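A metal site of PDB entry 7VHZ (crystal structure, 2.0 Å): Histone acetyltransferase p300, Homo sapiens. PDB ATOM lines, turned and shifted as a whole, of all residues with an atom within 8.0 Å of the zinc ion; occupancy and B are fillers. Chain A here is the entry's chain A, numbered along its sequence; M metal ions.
The side-chain sulfur (SG) of Cys 91 sits close to the backbone NH (N) of Glu 93. The backbone NH of Cys 91 is in hydrogen-bond range of the backbone carbonyl oxygen of Arg 96 (3.0 Å). N of Gly 118 lies close to SG of Cys 116 (3.3 Å). The side-chain sulfur (SG) of Cys 119 lies close to the side-chain carboxylate (OE1) of Glu 93 (3.7 Å).
Within 4 Å of the zinc ion: Cys 91, Cys 94, Cys 116 and Cys 119.
SG of Cys 94 binds the zinc ion (2.3 Å). SG of Cys 116 binds the zinc ion (2.3 Å). The zinc ion is bound by SG of Cys 91 (2.3 Å). The zinc ion is bound by SG of Cys 119 (2.3 Å). The zinc ion has four donor atoms within binding distance.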
ATOM      1  N   GLU A  90     -16.899   0.183 -27.466  1.00  0.00           N
ATOM      2  CA  GLU A  90     -16.799   0.773 -26.148  1.00  0.00           C
ATOM      3  C   GLU A  90     -15.624   0.172 -25.402  1.00  0.00           C
ATOM      4  O   GLU A  90     -15.493  -1.058 -25.321  1.00  0.00           O
ATOM      5  CB  GLU A  90     -18.097   0.562 -25.350  1.00  0.00           C
ATOM      6  CG  GLU A  90     -18.345   1.614 -24.286  1.00  0.00           C
ATOM      7  CD  GLU A  90     -19.615   1.353 -23.502  1.00  0.00           C
ATOM      8  OE1 GLU A  90     -20.513   2.227 -23.499  1.00  0.00           O
ATOM      9  OE2 GLU A  90     -19.722   0.273 -22.878  1.00  0.00           O
ATOM     10  N   CYS A  91     -14.764   1.033 -24.855  1.00  0.00           N
ATOM     11  CA  CYS A  91     -13.661   0.584 -24.036  1.00  0.00           C
ATOM     12  C   CYS A  91     -14.181  -0.177 -22.821  1.00  0.00           C
ATOM     13  O   CYS A  91     -15.087   0.280 -22.127  1.00  0.00           O
ATOM     14  CB  CYS A  91     -12.825   1.791 -23.587  1.00  0.00           C
ATOM     15  SG  CYS A  91     -11.441   1.388 -22.479  1.00  0.00           S
ATOM     16  N   THR A  92     -13.598  -1.352 -22.569  1.00  0.00           N
ATOM     17  CA  THR A  92     -14.058  -2.180 -21.462  1.00  0.00           C
ATOM     18  C   THR A  92     -13.686  -1.593 -20.111  1.00  0.00           C
ATOM     19  O   THR A  92     -14.066  -2.165 -19.077  1.00  0.00           O
ATOM     20  CB  THR A  92     -13.523  -3.611 -21.599  1.00  0.00           C
ATOM     21  OG1 THR A  92     -12.100  -3.567 -21.810  1.00  0.00           O
ATOM     22  CG2 THR A  92     -14.185  -4.320 -22.776  1.00  0.00           C
ATOM     23  N   GLU A  93     -12.909  -0.516 -20.082  1.00  0.00           N
ATOM     24  CA  GLU A  93     -12.540   0.155 -18.835  1.00  0.00           C
ATOM     25  C   GLU A  93     -13.036   1.595 -18.774  1.00  0.00           C
ATOM     26  O   GLU A  93     -13.643   1.984 -17.769  1.00  0.00           O
ATOM     27  CB  GLU A  93     -11.020   0.111 -18.643  1.00  0.00           C
ATOM     28  CG  GLU A  93     -10.473  -1.291 -18.708  1.00  0.00           C
ATOM     29  CD  GLU A  93      -8.964  -1.323 -18.586  1.00  0.00           C
ATOM     30  OE1 GLU A  93      -8.382  -0.292 -18.213  1.00  0.00           O
ATOM     31  OE2 GLU A  93      -8.371  -2.382 -18.861  1.00  0.00           O
ATOM     32  N   CYS A  94     -12.857   2.372 -19.841  1.00  0.00           N
ATOM     33  CA  CYS A  94     -13.287   3.762 -19.806  1.00  0.00           C
ATOM     34  C   CYS A  94     -14.787   3.889 -19.966  1.00  0.00           C
ATOM     35  O   CYS A  94     -15.402   4.769 -19.368  1.00  0.00           O
ATOM     36  CB  CYS A  94     -12.663   4.548 -20.958  1.00  0.00           C
ATOM     37  SG  CYS A  94     -11.017   5.188 -20.812  1.00  0.00           S
ATOM     38  N   GLY A  95     -15.374   2.991 -20.745  1.00  0.00           N
ATOM     39  CA  GLY A  95     -16.703   3.220 -21.256  1.00  0.00           C
ATOM     40  C   GLY A  95     -16.695   4.180 -22.428  1.00  0.00           C
ATOM     41  O   GLY A  95     -17.763   4.523 -22.941  1.00  0.00           O
ATOM     42  N   ARG A  96     -15.509   4.642 -22.843  1.00  0.00           N
ATOM     43  CA  ARG A  96     -15.395   5.583 -23.946  1.00  0.00           C
ATOM     44  C   ARG A  96     -15.807   4.935 -25.259  1.00  0.00           C
ATOM     45  O   ARG A  96     -15.387   3.823 -25.585  1.00  0.00           O
ATOM     46  CB  ARG A  96     -13.949   6.103 -24.039  1.00  0.00           C
ATOM     47  N   LYS A  97     -16.641   5.635 -26.016  1.00  0.00           N
ATOM     48  CA  LYS A  97     -17.128   5.142 -27.299  1.00  0.00           C
ATOM     49  C   LYS A  97     -16.247   5.713 -28.406  1.00  0.00           C
ATOM     50  O   LYS A  97     -16.092   6.938 -28.514  1.00  0.00           O
ATOM     51  CB  LYS A  97     -18.593   5.522 -27.508  1.00  0.00           C
ATOM     52  N   MET A  98     -15.682   4.832 -29.229  1.00  0.00           N
ATOM     53  CA  MET A  98     -14.832   5.229 -30.340  1.00  0.00           C
ATOM     54  C   MET A  98     -15.220   4.453 -31.583  1.00  0.00           C
ATOM     55  O   MET A  98     -15.636   3.292 -31.502  1.00  0.00           O
ATOM     56  CB  MET A  98     -13.335   4.994 -30.028  1.00  0.00           C
ATOM     57  CG  MET A  98     -12.903   5.434 -28.623  1.00  0.00           C
ATOM     58  SD  MET A  98     -11.821   6.877 -28.615  1.00  0.00           S
ATOM     59  CE  MET A  98     -10.257   6.142 -29.062  1.00  0.00           C
ATOM     60  N   PHE A 114     -12.256  -4.624 -26.323  1.00  0.00           N
ATOM     61  CA  PHE A 114     -11.571  -3.393 -26.677  1.00  0.00           C
ATOM     62  C   PHE A 114     -11.123  -2.670 -25.415  1.00  0.00           C
ATOM     63  O   PHE A 114     -11.945  -2.333 -24.557  1.00  0.00           O
ATOM     64  CB  PHE A 114     -12.462  -2.477 -27.509  1.00  0.00           C
ATOM     65  CG  PHE A 114     -11.836  -1.129 -27.782  1.00  0.00           C
ATOM     66  CD1 PHE A 114     -10.591  -1.045 -28.385  1.00  0.00           C
ATOM     67  CD2 PHE A 114     -12.484   0.032 -27.412  1.00  0.00           C
ATOM     68  CE1 PHE A 114     -10.010   0.186 -28.639  1.00  0.00           C
ATOM     69  CE2 PHE A 114     -11.912   1.273 -27.660  1.00  0.00           C
ATOM     70  CZ  PHE A 114     -10.670   1.349 -28.275  1.00  0.00           C
ATOM     71  N   VAL A 115      -9.813  -2.427 -25.315  1.00  0.00           N
ATOM     72  CA  VAL A 115      -9.249  -1.532 -24.309  1.00  0.00           C
ATOM     73  C   VAL A 115      -8.575  -0.390 -25.062  1.00  0.00           C
ATOM     74  O   VAL A 115      -7.694  -0.624 -25.895  1.00  0.00           O
ATOM     75  CB  VAL A 115      -8.256  -2.256 -23.380  1.00  0.00           C
ATOM     76  CG1 VAL A 115      -7.685  -1.285 -22.352  1.00  0.00           C
ATOM     77  CG2 VAL A 115      -8.921  -3.441 -22.699  1.00  0.00           C
ATOM     78  N   CYS A 116      -8.988   0.840 -24.745  1.00  0.00           N
ATOM     79  CA  CYS A 116      -8.556   2.005 -25.501  1.00  0.00           C
ATOM     80  C   CYS A 116      -7.089   2.332 -25.203  1.00  0.00           C
ATOM     81  O   CYS A 116      -6.466   1.800 -24.279  1.00  0.00           O
ATOM     82  CB  CYS A 116      -9.441   3.203 -25.185  1.00  0.00           C
ATOM     83  SG  CYS A 116      -8.927   4.148 -23.740  1.00  0.00           S
ATOM     84  N   ASP A 117      -6.525   3.197 -26.045  1.00  0.00           N
ATOM     85  CA  ASP A 117      -5.121   3.568 -25.911  1.00  0.00           C
ATOM     86  C   ASP A 117      -4.839   4.252 -24.576  1.00  0.00           C
ATOM     87  O   ASP A 117      -3.805   3.990 -23.937  1.00  0.00           O
ATOM     88  CB  ASP A 117      -4.695   4.484 -27.055  1.00  0.00           C
ATOM     89  CG  ASP A 117      -4.288   3.725 -28.305  1.00  0.00           C
ATOM     90  OD1 ASP A 117      -4.101   2.495 -28.209  1.00  0.00           O
ATOM     91  OD2 ASP A 117      -4.160   4.359 -29.370  1.00  0.00           O
ATOM     92  N   GLY A 118      -5.751   5.107 -24.123  1.00  0.00           N
ATOM     93  CA  GLY A 118      -5.562   5.786 -22.848  1.00  0.00           C
ATOM     94  C   GLY A 118      -5.455   4.826 -21.680  1.00  0.00           C
ATOM     95  O   GLY A 118      -4.570   4.935 -20.838  1.00  0.00           O
ATOM     96  N   CYS A 119      -6.375   3.854 -21.628  1.00  0.00           N
ATOM     97  CA  CYS A 119      -6.313   2.826 -20.600  1.00  0.00           C
ATOM     98  C   CYS A 119      -5.085   1.947 -20.755  1.00  0.00           C
ATOM     99  O   CYS A 119      -4.623   1.351 -19.779  1.00  0.00           O
ATOM    100  CB  CYS A 119      -7.581   1.977 -20.617  1.00  0.00           C
ATOM    101  SG  CYS A 119      -9.046   2.858 -20.055  1.00  0.00           S
ATOM    102  N   LEU A 120      -4.571   1.832 -21.981  1.00  0.00           N
ATOM    103  CA  LEU A 120      -3.342   1.076 -22.195  1.00  0.00           C
ATOM    104  C   LEU A 120      -2.138   1.815 -21.622  1.00  0.00           C
ATOM    105  O   LEU A 120      -1.305   1.219 -20.930  1.00  0.00           O
ATOM    106  CB  LEU A 120      -3.151   0.795 -23.681  1.00  0.00           C
ATOM    107  CG  LEU A 120      -3.962  -0.378 -24.248  1.00  0.00           C
ATOM    108  CD1 LEU A 120      -3.570  -0.657 -25.698  1.00  0.00           C
ATOM    109  CD2 LEU A 120      -3.772  -1.629 -23.389  1.00  0.00           C
HETATM  110 ZN    ZN M   1     -10.258   3.343 -22.005  1.00  0.00          ZN
